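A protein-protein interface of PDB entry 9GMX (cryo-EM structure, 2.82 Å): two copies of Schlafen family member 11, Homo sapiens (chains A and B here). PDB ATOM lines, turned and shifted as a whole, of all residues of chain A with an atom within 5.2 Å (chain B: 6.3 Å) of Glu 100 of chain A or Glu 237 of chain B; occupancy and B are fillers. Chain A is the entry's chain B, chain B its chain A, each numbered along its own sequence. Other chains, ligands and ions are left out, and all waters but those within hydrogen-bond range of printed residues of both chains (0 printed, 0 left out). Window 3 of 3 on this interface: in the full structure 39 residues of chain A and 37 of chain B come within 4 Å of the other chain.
The guanidinium group (NH2) of Arg 283 of chain B lies within hydrogen-bond range of the backbone carbonyl oxygen (O) of Pro 98 of chain A, 3.2 Å away.
NE of Arg 163 of chain B sits at hydrogen-bond distance from O of Glu 165 of chain B (3.1 Å). The backbone NH (N) of Glu 165 of chain B lies within hydrogen-bond range of the side-chain amide oxygen (OE1) of Gln 239 of chain B, 2.7 Å away. OE2 of Glu 237 of chain B lies close to N of Phe 243 of chain B, at 2.7 Å. N of Gly 55 of chain A lies within hydrogen-bond range of O of Glu 100 of chain A (3.0 Å). OE2 of Glu 100 of chain A sits at hydrogen-bond distance from N of Glu 56 of chain A (2.9 Å).
Pro 236 of chain B touches Pro 98 of chain A. Glu 100 of chain A touches Pro 236 of chain B (OE1 to CB, 3.6 Å). Glu 100 of chain A touches Glu 237 of chain B. Met 101 of chain A touches Glu 165 of chain B.
Glu 237 of chain B touches one residue of chain A. Printed residues of chain A within 4 Å of Glu 165 of chain B: Met 101 (3.9 Å). Printed residues of chain B within 4 Å of Met 101 of chain A: Glu 165. The nearest printed residue of chain A that does not touch Glu 237 of chain B is Val 99 of chain A (5.7 Å). The nearest printed residue of chain A that does not touch Pro 236 of chain B is Val 99 of chain A (4.02 Å).
Of the 9 printed residues of chain A, 3 touch a printed residue of chain B. Printed residues of chain A that touch a printed residue of chain B: Pro 98, Glu 100 and Met 101. Hydrophobic or aromatic side chains of chain A within 4 Å of the printed part of chain B: Pro 98 and Met 101. Printed residues of chain B that touch a printed residue of chain A: Glu 165, Pro 236, Glu 237 and Arg 283. Hydrophobic or aromatic side chains of chain B that line the printed part of chain A: Pro 236. Among the printed residues, 5 pairs touch across the chains.
No position is printed for both chains. Of the 5 pairs that touch across the chains among the printed residues, none has its exchanged pair printed and touching as well.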
ATOM      1  N   LEU A  54      -7.865  21.444  16.166  1.00  0.00           N
ATOM      2  CA  LEU A  54      -7.210  20.564  17.110  1.00  0.00           C
ATOM      3  C   LEU A  54      -7.363  21.147  18.503  1.00  0.00           C
ATOM      4  O   LEU A  54      -7.651  22.332  18.673  1.00  0.00           O
ATOM      5  CB  LEU A  54      -5.735  20.381  16.752  1.00  0.00           C
ATOM      6  CG  LEU A  54      -5.478  19.809  15.358  1.00  0.00           C
ATOM      7  CD1 LEU A  54      -4.039  19.989  14.982  1.00  0.00           C
ATOM      8  CD2 LEU A  54      -5.870  18.356  15.282  1.00  0.00           C
ATOM      9  N   GLY A  55      -7.171  20.297  19.502  1.00  0.00           N
ATOM     10  CA  GLY A  55      -7.459  20.661  20.871  1.00  0.00           C
ATOM     11  C   GLY A  55      -8.855  20.216  21.245  1.00  0.00           C
ATOM     12  O   GLY A  55      -9.791  20.389  20.464  1.00  0.00           O
ATOM     13  N   GLU A  56      -9.013  19.623  22.425  1.00  0.00           N
ATOM     14  CA  GLU A  56     -10.331  19.144  22.826  1.00  0.00           C
ATOM     15  C   GLU A  56     -11.265  20.307  23.133  1.00  0.00           C
ATOM     16  O   GLU A  56     -12.447  20.275  22.782  1.00  0.00           O
ATOM     17  CB  GLU A  56     -10.195  18.202  24.021  1.00  0.00           C
ATOM     18  CG  GLU A  56     -11.506  17.700  24.609  1.00  0.00           C
ATOM     19  CD  GLU A  56     -12.382  16.942  23.620  1.00  0.00           C
ATOM     20  OE1 GLU A  56     -11.992  16.789  22.446  1.00  0.00           O
ATOM     21  OE2 GLU A  56     -13.463  16.474  24.036  1.00  0.00           O
ATOM     22  N   GLU A  57     -10.749  21.358  23.768  1.00  0.00           N
ATOM     23  CA  GLU A  57     -11.585  22.524  24.037  1.00  0.00           C
ATOM     24  C   GLU A  57     -12.061  23.168  22.744  1.00  0.00           C
ATOM     25  O   GLU A  57     -13.228  23.555  22.627  1.00  0.00           O
ATOM     26  CB  GLU A  57     -10.829  23.541  24.892  1.00  0.00           C
ATOM     27  CG  GLU A  57      -9.921  22.935  25.935  1.00  0.00           C
ATOM     28  CD  GLU A  57     -10.668  22.030  26.887  1.00  0.00           C
ATOM     29  OE1 GLU A  57     -10.013  21.236  27.596  1.00  0.00           O
ATOM     30  OE2 GLU A  57     -11.911  22.121  26.935  1.00  0.00           O
ATOM     31  N   PRO A  98       1.144  24.966  20.990  1.00  0.00           N
ATOM     32  CA  PRO A  98       0.973  23.512  21.004  1.00  0.00           C
ATOM     33  C   PRO A  98      -0.391  23.125  21.550  1.00  0.00           C
ATOM     34  O   PRO A  98      -0.860  23.674  22.545  1.00  0.00           O
ATOM     35  CB  PRO A  98       2.102  23.037  21.921  1.00  0.00           C
ATOM     36  CG  PRO A  98       3.083  24.129  21.918  1.00  0.00           C
ATOM     37  CD  PRO A  98       2.305  25.382  21.789  1.00  0.00           C
ATOM     38  N   VAL A  99      -1.021  22.153  20.904  1.00  0.00           N
ATOM     39  CA  VAL A  99      -2.317  21.660  21.338  1.00  0.00           C
ATOM     40  C   VAL A  99      -2.272  20.144  21.338  1.00  0.00           C
ATOM     41  O   VAL A  99      -1.390  19.529  20.735  1.00  0.00           O
ATOM     42  CB  VAL A  99      -3.470  22.158  20.444  1.00  0.00           C
ATOM     43  CG1 VAL A  99      -3.598  23.657  20.545  1.00  0.00           C
ATOM     44  CG2 VAL A  99      -3.268  21.718  19.010  1.00  0.00           C
ATOM     45  N   GLU A 100      -3.215  19.544  22.051  1.00  0.00           N
ATOM     46  CA  GLU A 100      -3.409  18.112  21.963  1.00  0.00           C
ATOM     47  C   GLU A 100      -4.246  17.741  20.741  1.00  0.00           C
ATOM     48  O   GLU A 100      -4.825  18.592  20.071  1.00  0.00           O
ATOM     49  CB  GLU A 100      -4.054  17.576  23.244  1.00  0.00           C
ATOM     50  CG  GLU A 100      -5.487  18.032  23.492  1.00  0.00           C
ATOM     51  CD  GLU A 100      -5.582  19.420  24.096  1.00  0.00           C
ATOM     52  OE1 GLU A 100      -4.556  19.947  24.557  1.00  0.00           O
ATOM     53  OE2 GLU A 100      -6.684  19.998  24.083  1.00  0.00           O
ATOM     54  N   MET A 101      -4.289  16.454  20.442  1.00  0.00           N
ATOM     55  CA  MET A 101      -4.978  16.024  19.236  1.00  0.00           C
ATOM     56  C   MET A 101      -6.492  16.154  19.370  1.00  0.00           C
ATOM     57  O   MET A 101      -7.172  16.510  18.404  1.00  0.00           O
ATOM     58  CB  MET A 101      -4.555  14.594  18.910  1.00  0.00           C
ATOM     59  CG  MET A 101      -5.130  14.042  17.627  1.00  0.00           C
ATOM     60  SD  MET A 101      -4.535  12.398  17.193  1.00  0.00           S
ATOM     61  CE  MET A 101      -2.916  12.730  16.522  1.00  0.00           C
ATOM     62  N   GLY A 102      -7.036  15.867  20.548  1.00  0.00           N
ATOM     63  CA  GLY A 102      -8.473  15.837  20.731  1.00  0.00           C
ATOM     64  C   GLY A 102      -8.930  14.422  21.008  1.00  0.00           C
ATOM     65  O   GLY A 102      -8.466  13.472  20.373  1.00  0.00           O
ATOM     66  N   ARG B 163      -1.347   4.570  29.323  1.00  0.00           N
ATOM     67  CA  ARG B 163      -1.500   5.938  28.868  1.00  0.00           C
ATOM     68  C   ARG B 163      -1.617   5.877  27.349  1.00  0.00           C
ATOM     69  O   ARG B 163      -0.782   5.272  26.677  1.00  0.00           O
ATOM     70  CB  ARG B 163      -0.335   6.826  29.284  1.00  0.00           C
ATOM     71  CG  ARG B 163      -0.467   8.274  28.981  1.00  0.00           C
ATOM     72  CD  ARG B 163      -1.381   8.974  29.923  1.00  0.00           C
ATOM     73  NE  ARG B 163      -1.288  10.413  29.738  1.00  0.00           N
ATOM     74  CZ  ARG B 163      -2.075  11.293  30.329  1.00  0.00           C
ATOM     75  NH1 ARG B 163      -3.026  10.915  31.159  1.00  0.00           N
ATOM     76  NH2 ARG B 163      -1.914  12.584  30.066  1.00  0.00           N
ATOM     77  N   GLU B 165      -1.963   8.688  24.636  1.00  0.00           N
ATOM     78  CA  GLU B 165      -1.978  10.130  24.439  1.00  0.00           C
ATOM     79  C   GLU B 165      -2.429  10.811  25.723  1.00  0.00           C
ATOM     80  O   GLU B 165      -1.732  10.729  26.733  1.00  0.00           O
ATOM     81  CB  GLU B 165      -2.869  10.513  23.258  1.00  0.00           C
ATOM     82  CG  GLU B 165      -2.232  10.307  21.917  1.00  0.00           C
ATOM     83  CD  GLU B 165      -1.400  11.493  21.493  1.00  0.00           C
ATOM     84  OE1 GLU B 165      -1.989  12.511  21.073  1.00  0.00           O
ATOM     85  OE2 GLU B 165      -0.159  11.417  21.580  1.00  0.00           O
ATOM     86  N   THR B 166      -3.577  11.479  25.714  1.00  0.00           N
ATOM     87  CA  THR B 166      -4.030  12.242  26.866  1.00  0.00           C
ATOM     88  C   THR B 166      -5.085  11.517  27.685  1.00  0.00           C
ATOM     89  O   THR B 166      -5.804  12.166  28.447  1.00  0.00           O
ATOM     90  CB  THR B 166      -4.582  13.601  26.426  1.00  0.00           C
ATOM     91  OG1 THR B 166      -5.756  13.410  25.633  1.00  0.00           O
ATOM     92  CG2 THR B 166      -3.560  14.373  25.632  1.00  0.00           C
ATOM     93  N   PHE B 235       2.593  24.159  28.025  1.00  0.00           N
ATOM     94  CA  PHE B 235       2.504  22.928  27.258  1.00  0.00           C
ATOM     95  C   PHE B 235       1.165  22.263  27.524  1.00  0.00           C
ATOM     96  O   PHE B 235       0.570  22.465  28.589  1.00  0.00           O
ATOM     97  CB  PHE B 235       3.648  21.962  27.607  1.00  0.00           C
ATOM     98  CG  PHE B 235       3.905  21.825  29.072  1.00  0.00           C
ATOM     99  CD1 PHE B 235       4.743  22.703  29.723  1.00  0.00           C
ATOM    100  CD2 PHE B 235       3.313  20.821  29.801  1.00  0.00           C
ATOM    101  CE1 PHE B 235       4.983  22.582  31.068  1.00  0.00           C
ATOM    102  CE2 PHE B 235       3.553  20.698  31.146  1.00  0.00           C
ATOM    103  CZ  PHE B 235       4.387  21.581  31.780  1.00  0.00           C
ATOM    104  N   PRO B 236       0.663  21.479  26.579  1.00  0.00           N
ATOM    105  CA  PRO B 236      -0.608  20.788  26.783  1.00  0.00           C
ATOM    106  C   PRO B 236      -0.405  19.433  27.441  1.00  0.00           C
ATOM    107  O   PRO B 236       0.714  18.978  27.668  1.00  0.00           O
ATOM    108  CB  PRO B 236      -1.130  20.630  25.361  1.00  0.00           C
ATOM    109  CG  PRO B 236       0.094  20.417  24.582  1.00  0.00           C
ATOM    110  CD  PRO B 236       1.163  21.264  25.215  1.00  0.00           C
ATOM    111  N   GLU B 237      -1.524  18.786  27.743  1.00  0.00           N
ATOM    112  CA  GLU B 237      -1.476  17.393  28.147  1.00  0.00           C
ATOM    113  C   GLU B 237      -1.040  16.526  26.977  1.00  0.00           C
ATOM    114  O   GLU B 237      -1.409  16.765  25.827  1.00  0.00           O
ATOM    115  CB  GLU B 237      -2.836  16.934  28.649  1.00  0.00           C
ATOM    116  CG  GLU B 237      -3.214  17.481  29.984  1.00  0.00           C
ATOM    117  CD  GLU B 237      -4.500  16.896  30.474  1.00  0.00           C
ATOM    118  OE1 GLU B 237      -5.338  16.555  29.623  1.00  0.00           O
ATOM    119  OE2 GLU B 237      -4.687  16.788  31.700  1.00  0.00           O
ATOM    120  N   SER B 238      -0.251  15.508  27.280  1.00  0.00           N
ATOM    121  CA  SER B 238       0.281  14.629  26.253  1.00  0.00           C
ATOM    122  C   SER B 238       0.554  13.271  26.880  1.00  0.00           C
ATOM    123  O   SER B 238       0.283  13.047  28.061  1.00  0.00           O
ATOM    124  CB  SER B 238       1.540  15.232  25.627  1.00  0.00           C
ATOM    125  OG  SER B 238       2.649  15.116  26.493  1.00  0.00           O
ATOM    126  N   GLN B 239       1.116  12.369  26.082  1.00  0.00           N
ATOM    127  CA  GLN B 239       1.475  11.035  26.540  1.00  0.00           C
ATOM    128  C   GLN B 239       2.292  11.059  27.824  1.00  0.00           C
ATOM    129  O   GLN B 239       2.359  10.047  28.522  1.00  0.00           O
ATOM    130  CB  GLN B 239       2.256  10.343  25.426  1.00  0.00           C
ATOM    131  CG  GLN B 239       2.684   8.922  25.681  1.00  0.00           C
ATOM    132  CD  GLN B 239       1.596   7.935  25.423  1.00  0.00           C
ATOM    133  OE1 GLN B 239       0.714   8.165  24.607  1.00  0.00           O
ATOM    134  NE2 GLN B 239       1.665   6.806  26.095  1.00  0.00           N
ATOM    135  N   LEU B 240       2.912  12.179  28.155  1.00  0.00           N
ATOM    136  CA  LEU B 240       3.795  12.267  29.304  1.00  0.00           C
ATOM    137  C   LEU B 240       3.328  13.254  30.356  1.00  0.00           C
ATOM    138  O   LEU B 240       4.008  13.403  31.373  1.00  0.00           O
ATOM    139  CB  LEU B 240       5.204  12.667  28.849  1.00  0.00           C
ATOM    140  CG  LEU B 240       5.874  11.728  27.850  1.00  0.00           C
ATOM    141  CD1 LEU B 240       6.990  12.443  27.146  1.00  0.00           C
ATOM    142  CD2 LEU B 240       6.400  10.492  28.547  1.00  0.00           C
ATOM    143  N   VAL B 241       2.204  13.933  30.147  1.00  0.00           N
ATOM    144  CA  VAL B 241       1.759  15.011  31.023  1.00  0.00           C
ATOM    145  C   VAL B 241       0.274  14.852  31.278  1.00  0.00           C
ATOM    146  O   VAL B 241      -0.488  14.549  30.356  1.00  0.00           O
ATOM    147  CB  VAL B 241       2.047  16.397  30.418  1.00  0.00           C
ATOM    148  CG1 VAL B 241       1.319  17.462  31.184  1.00  0.00           C
ATOM    149  CG2 VAL B 241       3.531  16.675  30.415  1.00  0.00           C
ATOM    150  N   GLU B 242      -0.138  15.050  32.526  1.00  0.00           N
ATOM    151  CA  GLU B 242      -1.539  15.046  32.916  1.00  0.00           C
ATOM    152  C   GLU B 242      -1.787  16.194  33.878  1.00  0.00           C
ATOM    153  O   GLU B 242      -1.042  16.375  34.844  1.00  0.00           O
ATOM    154  CB  GLU B 242      -1.935  13.713  33.567  1.00  0.00           C
ATOM    155  CG  GLU B 242      -3.330  13.670  34.152  1.00  0.00           C
ATOM    156  CD  GLU B 242      -4.402  13.697  33.107  1.00  0.00           C
ATOM    157  OE1 GLU B 242      -4.226  13.042  32.070  1.00  0.00           O
ATOM    158  OE2 GLU B 242      -5.416  14.390  33.304  1.00  0.00           O
ATOM    159  N   PHE B 243      -2.838  16.962  33.613  1.00  0.00           N
ATOM    160  CA  PHE B 243      -3.262  18.060  34.469  1.00  0.00           C
ATOM    161  C   PHE B 243      -4.519  17.652  35.217  1.00  0.00           C
ATOM    162  O   PHE B 243      -5.494  17.211  34.603  1.00  0.00           O
ATOM    163  CB  PHE B 243      -3.545  19.324  33.660  1.00  0.00           C
ATOM    164  CG  PHE B 243      -2.358  19.868  32.934  1.00  0.00           C
ATOM    165  CD1 PHE B 243      -1.099  19.814  33.492  1.00  0.00           C
ATOM    166  CD2 PHE B 243      -2.507  20.448  31.694  1.00  0.00           C
ATOM    167  CE1 PHE B 243      -0.020  20.323  32.830  1.00  0.00           C
ATOM    168  CE2 PHE B 243      -1.430  20.956  31.030  1.00  0.00           C
ATOM    169  CZ  PHE B 243      -0.182  20.895  31.600  1.00  0.00           C
ATOM    170  N   LYS B 244      -4.493  17.807  36.536  1.00  0.00           N
ATOM    171  CA  LYS B 244      -5.623  17.515  37.401  1.00  0.00           C
ATOM    172  C   LYS B 244      -5.801  18.649  38.392  1.00  0.00           C
ATOM    173  O   LYS B 244      -4.824  19.151  38.947  1.00  0.00           O
ATOM    174  CB  LYS B 244      -5.414  16.205  38.183  1.00  0.00           C
ATOM    175  CG  LYS B 244      -5.675  14.898  37.453  1.00  0.00           C
ATOM    176  CD  LYS B 244      -6.998  14.870  36.726  1.00  0.00           C
ATOM    177  CE  LYS B 244      -7.884  13.778  37.262  1.00  0.00           C
ATOM    178  NZ  LYS B 244      -9.021  13.499  36.364  1.00  0.00           N
ATOM    179  N   ASP B 280      -7.438  21.727  33.913  1.00  0.00           N
ATOM    180  CA  ASP B 280      -7.299  20.861  32.752  1.00  0.00           C
ATOM    181  C   ASP B 280      -7.465  21.631  31.454  1.00  0.00           C
ATOM    182  O   ASP B 280      -6.851  21.283  30.443  1.00  0.00           O
ATOM    183  CB  ASP B 280      -8.332  19.738  32.843  1.00  0.00           C
ATOM    184  CG  ASP B 280      -7.936  18.518  32.066  1.00  0.00           C
ATOM    185  OD1 ASP B 280      -7.167  17.692  32.608  1.00  0.00           O
ATOM    186  OD2 ASP B 280      -8.408  18.372  30.921  1.00  0.00           O
ATOM    187  N   ARG B 283      -5.072  25.331  31.607  1.00  0.00           N
ATOM    188  CA  ARG B 283      -3.697  25.047  31.997  1.00  0.00           C
ATOM    189  C   ARG B 283      -3.198  25.992  33.078  1.00  0.00           C
ATOM    190  O   ARG B 283      -1.993  26.182  33.222  1.00  0.00           O
ATOM    191  CB  ARG B 283      -2.754  25.101  30.794  1.00  0.00           C
ATOM    192  CG  ARG B 283      -3.373  24.635  29.502  1.00  0.00           C
ATOM    193  CD  ARG B 283      -2.331  24.406  28.435  1.00  0.00           C
ATOM    194  NE  ARG B 283      -2.948  24.027  27.171  1.00  0.00           N
ATOM    195  CZ  ARG B 283      -2.322  24.005  26.002  1.00  0.00           C
ATOM    196  NH1 ARG B 283      -1.051  24.349  25.892  1.00  0.00           N
ATOM    197  NH2 ARG B 283      -2.992  23.634  24.915  1.00  0.00           N
